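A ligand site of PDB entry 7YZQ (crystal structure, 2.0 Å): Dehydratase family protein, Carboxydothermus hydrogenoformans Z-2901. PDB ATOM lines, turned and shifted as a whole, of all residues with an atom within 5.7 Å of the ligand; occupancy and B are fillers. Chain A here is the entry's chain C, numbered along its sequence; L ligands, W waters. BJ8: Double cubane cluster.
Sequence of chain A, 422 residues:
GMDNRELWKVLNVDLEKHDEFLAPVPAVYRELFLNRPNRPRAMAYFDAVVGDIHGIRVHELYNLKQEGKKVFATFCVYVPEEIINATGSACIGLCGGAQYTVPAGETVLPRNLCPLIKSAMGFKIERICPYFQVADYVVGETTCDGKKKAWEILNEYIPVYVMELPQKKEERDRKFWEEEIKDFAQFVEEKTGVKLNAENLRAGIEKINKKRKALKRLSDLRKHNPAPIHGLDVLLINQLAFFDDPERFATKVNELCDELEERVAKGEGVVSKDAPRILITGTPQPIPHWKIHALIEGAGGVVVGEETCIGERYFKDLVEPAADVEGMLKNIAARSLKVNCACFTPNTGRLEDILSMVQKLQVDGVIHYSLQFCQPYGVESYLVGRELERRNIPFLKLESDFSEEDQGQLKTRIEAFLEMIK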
ATOM      1  N   PHE A  75      16.536  -8.355  19.083  1.00  0.00           N
ATOM      2  CA  PHE A  75      17.322  -8.157  17.868  1.00  0.00           C
ATOM      3  C   PHE A  75      16.508  -7.662  16.695  1.00  0.00           C
ATOM      4  O   PHE A  75      17.048  -7.565  15.601  1.00  0.00           O
ATOM      5  CB  PHE A  75      18.017  -9.476  17.484  1.00  0.00           C
ATOM      6  CG  PHE A  75      18.937 -10.007  18.562  1.00  0.00           C
ATOM      7  CD1 PHE A  75      18.421 -10.709  19.642  1.00  0.00           C
ATOM      8  CD2 PHE A  75      20.272  -9.776  18.504  1.00  0.00           C
ATOM      9  CE1 PHE A  75      19.232 -11.192  20.657  1.00  0.00           C
ATOM     10  CE2 PHE A  75      21.119 -10.231  19.499  1.00  0.00           C
ATOM     11  CZ  PHE A  75      20.599 -10.944  20.587  1.00  0.00           C
ATOM     12  N   CYS A  76      15.234  -7.324  16.879  1.00  0.00           N
ATOM     13  CA  CYS A  76      14.357  -6.918  15.794  1.00  0.00           C
ATOM     14  C   CYS A  76      13.390  -5.867  16.309  1.00  0.00           C
ATOM     15  O   CYS A  76      12.980  -5.929  17.474  1.00  0.00           O
ATOM     16  CB  CYS A  76      13.593  -8.124  15.243  1.00  0.00           C
ATOM     17  SG  CYS A  76      12.294  -7.753  14.014  1.00  0.00           S
ATOM     18  N   VAL A  77      13.033  -4.899  15.463  1.00  0.00           N
ATOM     19  CA  VAL A  77      12.157  -3.826  15.897  1.00  0.00           C
ATOM     20  C   VAL A  77      10.747  -4.330  16.157  1.00  0.00           C
ATOM     21  O   VAL A  77       9.929  -3.584  16.715  1.00  0.00           O
ATOM     22  CB  VAL A  77      12.137  -2.677  14.872  1.00  0.00           C
ATOM     23  CG1 VAL A  77      13.547  -2.176  14.648  1.00  0.00           C
ATOM     24  CG2 VAL A  77      11.450  -3.166  13.559  1.00  0.00           C
ATOM     25  N   TYR A  78      10.439  -5.553  15.727  1.00  0.00           N
ATOM     26  CA  TYR A  78       9.114  -6.134  15.859  1.00  0.00           C
ATOM     27  C   TYR A  78       8.793  -6.549  17.284  1.00  0.00           C
ATOM     28  O   TYR A  78       7.607  -6.659  17.637  1.00  0.00           O
ATOM     29  CB  TYR A  78       8.994  -7.345  14.910  1.00  0.00           C
ATOM     30  CG  TYR A  78       8.387  -6.959  13.613  1.00  0.00           C
ATOM     31  CD1 TYR A  78       7.000  -6.997  13.453  1.00  0.00           C
ATOM     32  CD2 TYR A  78       9.159  -6.550  12.526  1.00  0.00           C
ATOM     33  CE1 TYR A  78       6.402  -6.637  12.253  1.00  0.00           C
ATOM     34  CE2 TYR A  78       8.543  -6.160  11.295  1.00  0.00           C
ATOM     35  CZ  TYR A  78       7.185  -6.197  11.180  1.00  0.00           C
ATOM     36  OH  TYR A  78       6.478  -5.807  10.011  1.00  0.00           O
ATOM     37  N   CYS A  95      21.624  -6.401  18.550  1.00  0.00           N
ATOM     38  CA  CYS A  95      22.200  -6.695  17.233  1.00  0.00           C
ATOM     39  C   CYS A  95      23.704  -6.399  17.203  1.00  0.00           C
ATOM     40  O   CYS A  95      24.130  -5.318  17.625  1.00  0.00           O
ATOM     41  CB  CYS A  95      21.504  -5.873  16.141  1.00  0.00           C
ATOM     42  SG  CYS A  95      19.880  -6.556  15.821  1.00  0.00           S
ATOM     43  N   CYS A 114      25.095 -13.851   7.870  1.00  0.00           N
ATOM     44  CA  CYS A 114      25.112 -12.431   8.179  1.00  0.00           C
ATOM     45  C   CYS A 114      26.077 -12.148   9.334  1.00  0.00           C
ATOM     46  O   CYS A 114      25.967 -12.773  10.397  1.00  0.00           O
ATOM     47  CB  CYS A 114      23.715 -11.936   8.554  1.00  0.00           C
ATOM     48  SG  CYS A 114      23.544 -10.250   8.971  1.00  0.00           S
ATOM     49  N   LEU A 116      25.852  -9.649  11.347  1.00  0.00           N
ATOM     50  CA  LEU A 116      25.075  -9.242  12.514  1.00  0.00           C
ATOM     51  C   LEU A 116      24.834 -10.434  13.428  1.00  0.00           C
ATOM     52  O   LEU A 116      24.957 -10.323  14.643  1.00  0.00           O
ATOM     53  CB  LEU A 116      23.756  -8.604  12.066  1.00  0.00           C
ATOM     54  CG  LEU A 116      22.839  -8.052  13.166  1.00  0.00           C
ATOM     55  CD1 LEU A 116      21.934  -6.998  12.553  1.00  0.00           C
ATOM     56  CD2 LEU A 116      22.054  -9.137  13.809  1.00  0.00           C
ATOM     57  N   ILE A 117      24.432 -11.550  12.870  1.00  0.00           N
ATOM     58  CA  ILE A 117      24.086 -12.720  13.669  1.00  0.00           C
ATOM     59  C   ILE A 117      25.345 -13.322  14.303  1.00  0.00           C
ATOM     60  O   ILE A 117      25.364 -13.691  15.477  1.00  0.00           O
ATOM     61  CB  ILE A 117      23.356 -13.751  12.797  1.00  0.00           C
ATOM     62  CG1 ILE A 117      22.202 -13.138  11.992  1.00  0.00           C
ATOM     63  CG2 ILE A 117      22.840 -14.876  13.710  1.00  0.00           C
ATOM     64  CD1 ILE A 117      21.603 -14.125  10.960  1.00  0.00           C
ATOM     65  N   GLU A 141      12.876 -13.725  17.028  1.00  0.00           N
ATOM     66  CA  GLU A 141      11.766 -13.654  16.100  1.00  0.00           C
ATOM     67  C   GLU A 141      12.109 -14.481  14.865  1.00  0.00           C
ATOM     68  O   GLU A 141      13.286 -14.595  14.488  1.00  0.00           O
ATOM     69  CB  GLU A 141      11.508 -12.192  15.743  1.00  0.00           C
ATOM     70  CG  GLU A 141      12.362 -11.663  14.589  1.00  0.00           C
ATOM     71  CD  GLU A 141      13.827 -11.393  14.919  1.00  0.00           C
ATOM     72  OE1 GLU A 141      14.237 -11.433  16.078  1.00  0.00           O
ATOM     73  OE2 GLU A 141      14.596 -11.036  13.967  1.00  0.00           O
ATOM     74  N   THR A 143      12.330 -14.188  11.543  1.00  0.00           N
ATOM     75  CA  THR A 143      12.528 -13.347  10.373  1.00  0.00           C
ATOM     76  C   THR A 143      13.442 -14.052   9.388  1.00  0.00           C
ATOM     77  O   THR A 143      12.977 -14.885   8.598  1.00  0.00           O
ATOM     78  CB  THR A 143      13.145 -11.998  10.743  1.00  0.00           C
ATOM     79  OG1 THR A 143      14.161 -12.211  11.740  1.00  0.00           O
ATOM     80  CG2 THR A 143      12.088 -11.053  11.263  1.00  0.00           C
ATOM     81  N   CYS A 144      14.741 -13.739   9.370  1.00  0.00           N
ATOM     82  CA  CYS A 144      15.605 -14.308   8.366  1.00  0.00           C
ATOM     83  C   CYS A 144      16.005 -15.693   8.807  1.00  0.00           C
ATOM     84  O   CYS A 144      15.704 -16.152   9.945  1.00  0.00           O
ATOM     85  CB  CYS A 144      16.859 -13.451   8.190  1.00  0.00           C
ATOM     86  SG  CYS A 144      17.702 -13.392   9.855  1.00  0.00           S
ATOM     87  N   LYS A 147      18.803 -16.002  11.705  1.00  0.00           N
ATOM     88  CA  LYS A 147      18.351 -15.679  13.050  1.00  0.00           C
ATOM     89  C   LYS A 147      17.470 -16.781  13.587  1.00  0.00           C
ATOM     90  O   LYS A 147      17.650 -17.224  14.734  1.00  0.00           O
ATOM     91  CB  LYS A 147      17.564 -14.360  13.018  1.00  0.00           C
ATOM     92  CG  LYS A 147      18.343 -13.100  13.309  1.00  0.00           C
ATOM     93  CD  LYS A 147      17.406 -11.917  13.039  1.00  0.00           C
ATOM     94  CE  LYS A 147      17.890 -10.718  13.730  1.00  0.00           C
ATOM     95  NZ  LYS A 147      16.865  -9.577  13.541  1.00  0.00           N
ATOM     96  N   GLY A 282      18.525  -0.234   3.224  1.00  0.00           N
ATOM     97  CA  GLY A 282      18.890  -1.647   3.332  1.00  0.00           C
ATOM     98  C   GLY A 282      18.791  -2.149   4.767  1.00  0.00           C
ATOM     99  O   GLY A 282      17.771  -1.944   5.451  1.00  0.00           O
ATOM    100  N   THR A 283      19.861  -2.818   5.225  1.00  0.00           N
ATOM    101  CA  THR A 283      19.905  -3.498   6.515  1.00  0.00           C
ATOM    102  C   THR A 283      20.295  -2.531   7.622  1.00  0.00           C
ATOM    103  O   THR A 283      20.831  -1.445   7.338  1.00  0.00           O
ATOM    104  CB  THR A 283      20.883  -4.667   6.460  1.00  0.00           C
ATOM    105  OG1 THR A 283      22.150  -4.227   5.957  1.00  0.00           O
ATOM    106  CG2 THR A 283      20.383  -5.778   5.532  1.00  0.00           C
ATOM    107  N   PRO A 284      19.947  -2.845   8.877  1.00  0.00           N
ATOM    108  CA  PRO A 284      20.420  -1.995   9.970  1.00  0.00           C
ATOM    109  C   PRO A 284      21.938  -2.016  10.108  1.00  0.00           C
ATOM    110  O   PRO A 284      22.619  -3.008   9.802  1.00  0.00           O
ATOM    111  CB  PRO A 284      19.755  -2.593  11.214  1.00  0.00           C
ATOM    112  CG  PRO A 284      19.528  -4.014  10.873  1.00  0.00           C
ATOM    113  CD  PRO A 284      19.206  -4.033   9.384  1.00  0.00           C
ATOM    114  N   CYS A 309      16.260  -0.300   9.852  1.00  0.00           N
ATOM    115  CA  CYS A 309      15.688  -0.454  11.195  1.00  0.00           C
ATOM    116  C   CYS A 309      16.544   0.163  12.281  1.00  0.00           C
ATOM    117  O   CYS A 309      16.085   0.237  13.426  1.00  0.00           O
ATOM    118  CB  CYS A 309      15.445  -1.920  11.482  1.00  0.00           C
ATOM    119  SG  CYS A 309      13.916  -2.530  10.715  1.00  0.00           S
ATOM    120  N   ARG A 313      12.804   2.964   9.717  1.00  0.00           N
ATOM    121  CA  ARG A 313      11.897   1.860   9.993  1.00  0.00           C
ATOM    122  C   ARG A 313      11.654   1.664  11.501  1.00  0.00           C
ATOM    123  O   ARG A 313      10.615   1.148  11.898  1.00  0.00           O
ATOM    124  CB  ARG A 313      12.448   0.552   9.429  1.00  0.00           C
ATOM    125  CG  ARG A 313      12.519   0.514   7.834  1.00  0.00           C
ATOM    126  CD  ARG A 313      12.478  -0.896   7.364  1.00  0.00           C
ATOM    127  NE  ARG A 313      13.654  -1.685   7.759  1.00  0.00           N
ATOM    128  CZ  ARG A 313      14.703  -1.908   6.982  1.00  0.00           C
ATOM    129  NH1 ARG A 313      14.776  -1.366   5.756  1.00  0.00           N
ATOM    130  NH2 ARG A 313      15.716  -2.638   7.462  1.00  0.00           N
ATOM    131  N   VAL A 339       6.088  -1.973   9.717  1.00  0.00           N
ATOM    132  CA  VAL A 339       7.500  -2.031   9.362  1.00  0.00           C
ATOM    133  C   VAL A 339       7.680  -2.894   8.121  1.00  0.00           C
ATOM    134  O   VAL A 339       7.350  -4.095   8.107  1.00  0.00           O
ATOM    135  CB  VAL A 339       8.314  -2.548  10.555  1.00  0.00           C
ATOM    136  CG1 VAL A 339       9.756  -2.889  10.129  1.00  0.00           C
ATOM    137  CG2 VAL A 339       8.278  -1.552  11.710  1.00  0.00           C
ATOM    138  N   CYS A 341       9.761  -4.703   6.305  1.00  0.00           N
ATOM    139  CA  CYS A 341      10.999  -5.466   6.271  1.00  0.00           C
ATOM    140  C   CYS A 341      10.971  -6.440   5.101  1.00  0.00           C
ATOM    141  O   CYS A 341       9.914  -6.934   4.709  1.00  0.00           O
ATOM    142  CB  CYS A 341      11.179  -6.228   7.588  1.00  0.00           C
ATOM    143  SG  CYS A 341      12.408  -7.551   7.563  1.00  0.00           S
ATOM    144  N   ALA A 342      12.153  -6.709   4.526  1.00  0.00           N
ATOM    145  CA  ALA A 342      12.248  -7.592   3.358  1.00  0.00           C
ATOM    146  C   ALA A 342      11.941  -9.039   3.667  1.00  0.00           C
ATOM    147  O   ALA A 342      11.809  -9.846   2.727  1.00  0.00           O
ATOM    148  CB  ALA A 342      13.676  -7.469   2.707  1.00  0.00           C
ATOM    149  N   CYS A 343      11.757  -9.399   4.938  1.00  0.00           N
ATOM    150  CA  CYS A 343      11.310 -10.748   5.257  1.00  0.00           C
ATOM    151  C   CYS A 343       9.832 -10.962   4.954  1.00  0.00           C
ATOM    152  O   CYS A 343       9.377 -12.096   4.881  1.00  0.00           O
ATOM    153  CB  CYS A 343      11.611 -11.077   6.739  1.00  0.00           C
ATOM    154  SG  CYS A 343      13.361 -11.103   7.142  1.00  0.00           S
ATOM    155  N   LEU A 371      24.239  -6.097   4.403  1.00  0.00           N
ATOM    156  CA  LEU A 371      25.344  -6.897   4.919  1.00  0.00           C
ATOM    157  C   LEU A 371      25.492  -8.132   4.061  1.00  0.00           C
ATOM    158  O   LEU A 371      24.510  -8.676   3.552  1.00  0.00           O
ATOM    159  CB  LEU A 371      25.100  -7.292   6.388  1.00  0.00           C
ATOM    160  CG  LEU A 371      24.995  -6.078   7.344  1.00  0.00           C
ATOM    161  CD1 LEU A 371      24.632  -6.575   8.823  1.00  0.00           C
ATOM    162  CD2 LEU A 371      26.262  -5.252   7.330  1.00  0.00           C
ATOM    163  N   PHE A 373      25.706 -11.791   2.891  1.00  0.00           N
ATOM    164  CA  PHE A 373      24.897 -12.980   3.144  1.00  0.00           C
ATOM    165  C   PHE A 373      23.547 -12.651   3.775  1.00  0.00           C
ATOM    166  O   PHE A 373      22.886 -13.583   4.286  1.00  0.00           O
ATOM    167  CB  PHE A 373      25.639 -14.009   4.006  1.00  0.00           C
ATOM    168  CG  PHE A 373      26.942 -14.412   3.438  1.00  0.00           C
ATOM    169  CD1 PHE A 373      26.982 -15.130   2.254  1.00  0.00           C
ATOM    170  CD2 PHE A 373      28.112 -14.050   4.039  1.00  0.00           C
ATOM    171  CE1 PHE A 373      28.198 -15.464   1.677  1.00  0.00           C
ATOM    172  CE2 PHE A 373      29.317 -14.406   3.463  1.00  0.00           C
ATOM    173  CZ  PHE A 373      29.343 -15.086   2.276  1.00  0.00           C
ATOM    174  N   CYS A 374      23.109 -11.389   3.760  1.00  0.00           N
ATOM    175  CA  CYS A 374      21.726 -11.096   4.143  1.00  0.00           C
ATOM    176  C   CYS A 374      20.924 -11.334   2.886  1.00  0.00           C
ATOM    177  O   CYS A 374      20.958 -10.528   1.941  1.00  0.00           O
ATOM    178  CB  CYS A 374      21.515  -9.677   4.640  1.00  0.00           C
ATOM    179  SG  CYS A 374      19.712  -9.307   4.755  1.00  0.00           S
ATOM    180  N   GLN A 375      20.226 -12.438   2.826  1.00  0.00           N
ATOM    181  CA  GLN A 375      19.570 -12.817   1.592  1.00  0.00           C
ATOM    182  C   GLN A 375      18.244 -12.080   1.403  1.00  0.00           C
ATOM    183  O   GLN A 375      17.911 -11.713   0.261  1.00  0.00           O
ATOM    184  CB  GLN A 375      19.341 -14.334   1.549  1.00  0.00           C
ATOM    185  CG  GLN A 375      20.549 -15.150   1.973  1.00  0.00           C
ATOM    186  CD  GLN A 375      21.693 -15.165   0.958  1.00  0.00           C
ATOM    187  OE1 GLN A 375      22.217 -14.110   0.537  1.00  0.00           O
ATOM    188  NE2 GLN A 375      22.125 -16.366   0.603  1.00  0.00           N
ATOM    189  N   PRO A 376      17.458 -11.818   2.463  1.00  0.00           N
ATOM    190  CA  PRO A 376      16.227 -11.014   2.253  1.00  0.00           C
ATOM    191  C   PRO A 376      16.521  -9.669   1.574  1.00  0.00           C
ATOM    192  O   PRO A 376      15.888  -9.341   0.552  1.00  0.00           O
ATOM    193  CB  PRO A 376      15.638 -10.881   3.664  1.00  0.00           C
ATOM    194  CG  PRO A 376      16.150 -12.110   4.395  1.00  0.00           C
ATOM    195  CD  PRO A 376      17.504 -12.392   3.823  1.00  0.00           C
ATOM    196  N   TYR A 377      17.487  -8.887   2.106  1.00  0.00           N
ATOM    197  CA  TYR A 377      17.775  -7.581   1.513  1.00  0.00           C
ATOM    198  C   TYR A 377      18.663  -7.710   0.268  1.00  0.00           C
ATOM    199  O   TYR A 377      18.551  -6.907  -0.678  1.00  0.00           O
ATOM    200  CB  TYR A 377      18.420  -6.639   2.556  1.00  0.00           C
ATOM    201  CG  TYR A 377      17.367  -6.190   3.533  1.00  0.00           C
ATOM    202  CD1 TYR A 377      16.614  -5.040   3.284  1.00  0.00           C
ATOM    203  CD2 TYR A 377      17.093  -6.941   4.693  1.00  0.00           C
ATOM    204  CE1 TYR A 377      15.579  -4.668   4.123  1.00  0.00           C
ATOM    205  CE2 TYR A 377      16.079  -6.565   5.535  1.00  0.00           C
ATOM    206  CZ  TYR A 377      15.352  -5.401   5.282  1.00  0.00           C
ATOM    207  OH  TYR A 377      14.316  -4.988   6.117  1.00  0.00           O
HETATM  208  S1  BJ8 L   1      20.451 -11.535   7.424  1.00  0.00           S
HETATM  209  S2  BJ8 L   1      17.516  -9.602   8.164  1.00  0.00           S
HETATM  210  S3  BJ8 L   1      20.130 -10.460  10.722  1.00  0.00           S
HETATM  211  S4  BJ8 L   1      20.716  -7.992   8.344  1.00  0.00           S
HETATM  212  S5  BJ8 L   1      15.253  -5.492  12.753  1.00  0.00           S
HETATM  213  S6  BJ8 L   1      15.524  -5.571   8.990  1.00  0.00           S
HETATM  214  S7  BJ8 L   1      14.611  -8.616  10.817  1.00  0.00           S
HETATM  215  S8  BJ8 L   1      12.190  -5.866  10.816  1.00  0.00           S
HETATM  216  S9  BJ8 L   1      18.151  -7.367  11.230  1.00  0.00           S
HETATM  217 FE1  BJ8 L   1      19.029  -8.708   9.635  1.00  0.00          FE
HETATM  218 FE2  BJ8 L   1      21.298 -10.060   8.924  1.00  0.00          FE
HETATM  219 FE3  BJ8 L   1      19.543  -9.510   7.092  1.00  0.00          FE
HETATM  220 FE4  BJ8 L   1      18.912 -11.300   9.046  1.00  0.00          FE
HETATM  221 FE5  BJ8 L   1      13.778  -7.001   9.469  1.00  0.00          FE
HETATM  222 FE6  BJ8 L   1      13.607  -6.996  12.235  1.00  0.00          FE
HETATM  223 FE7  BJ8 L   1      14.252  -4.781  10.813  1.00  0.00          FE
HETATM  224 FE8  BJ8 L   1      16.005  -6.823  10.916  1.00  0.00          FE
HETATM  225  O   HOH W   1      20.001 -14.960   7.634  1.00  0.00           O
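S6 of the ligand lies close to NH2 of Arg 313 (3.3 Å).
A sulfur (S7) of the ligand sits close to the side-chain hydroxyl (OG1) of Thr 143.
FE3 of the ligand is bound by SG of Cys 374, 2.4 Å away.
S5 of the ligand sits close to N of Val 77 (3.6 Å).
The side-chain sulfur of Cys 144 is bound to an iron atom (FE4) of the ligand (2.5 Å).
An iron atom (FE2) of the ligand is bound by the side-chain sulfur (SG) of Cys 114 (2.3 Å).
The side-chain sulfur of Cys 341 binds an iron atom (FE5) of the ligand (2.4 Å).
A sulfur (S9) of the ligand lies close to the side-chain amino group (NZ) of Lys 147 (3.4 Å).
FE6 of the ligand is bound by SG of Cys 76, 2.3 Å away.
The side-chain hydroxyl (OH) of Tyr 377 sits close to a sulfur (S6) of the ligand, 3.2 Å away.
The side-chain sulfur (SG) of Cys 309 binds an iron atom (FE7) of the ligand, at 2.3 Å.
O of Phe 75 touches S5 of the ligand, 3.95 Å away.
CD2 of Tyr 78 touches S8 of the ligand (3.5 Å).
Leu 116 touches the ligand.
CG1 of Ile 117 touches S3 of the ligand, 3.6 Å away.
Glu 141 touches the ligand.
CG2 of Thr 283 touches S4 of the ligand, 3.6 Å away.
CG of Pro 284 touches S9 of the ligand, 3.6 Å away.
Val 339 touches the ligand (CG1 to S8, 3.9 Å).
Hydrophobic or aromatic side chains that line the ligand: Val 77, Tyr 78, Leu 116, Ile 117, Pro 284, Val 339 and Tyr 377.
19 residues have an atom within 4 Å of the ligand: Phe 75, Cys 76, Val 77, Tyr 78, Cys 114, Leu 116, Ile 117, Glu 141, Thr 143, Cys 144, Lys 147, Thr 283, Pro 284, Cys 309, Arg 313, Val 339, Cys 341, Cys 374 and Tyr 377.
The nearest printed residue that does not touch the ligand is Leu 371 (4.2 Å).
The side-chain hydroxyl of Tyr 377 sits at hydrogen-bond distance from the backbone NH of Ala 342 (3.2 Å).
NZ of Lys 147 lies within salt-bridge range of OE2 of Glu 141 (2.7 Å).
SG of Cys 76 lies close to N of Tyr 78, 3.3 Å away.
The backbone carbonyl oxygen (O) of Phe 75 lies within hydrogen-bond range of the side-chain sulfur (SG) of Cys 95 (3.0 Å).
OH of Tyr 377 is in hydrogen-bond range of NH2 of Arg 313.
NH2 of Arg 313 sits at hydrogen-bond distance from O of Gly 282, at 3.0 Å.
The side-chain sulfur (SG) of Cys 341 sits close to the backbone NH (N) of Cys 343 (3.3 Å).
The side-chain sulfur (SG) of Cys 309 sits close to the guanidinium group (NE) of Arg 313 (3.1 Å).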
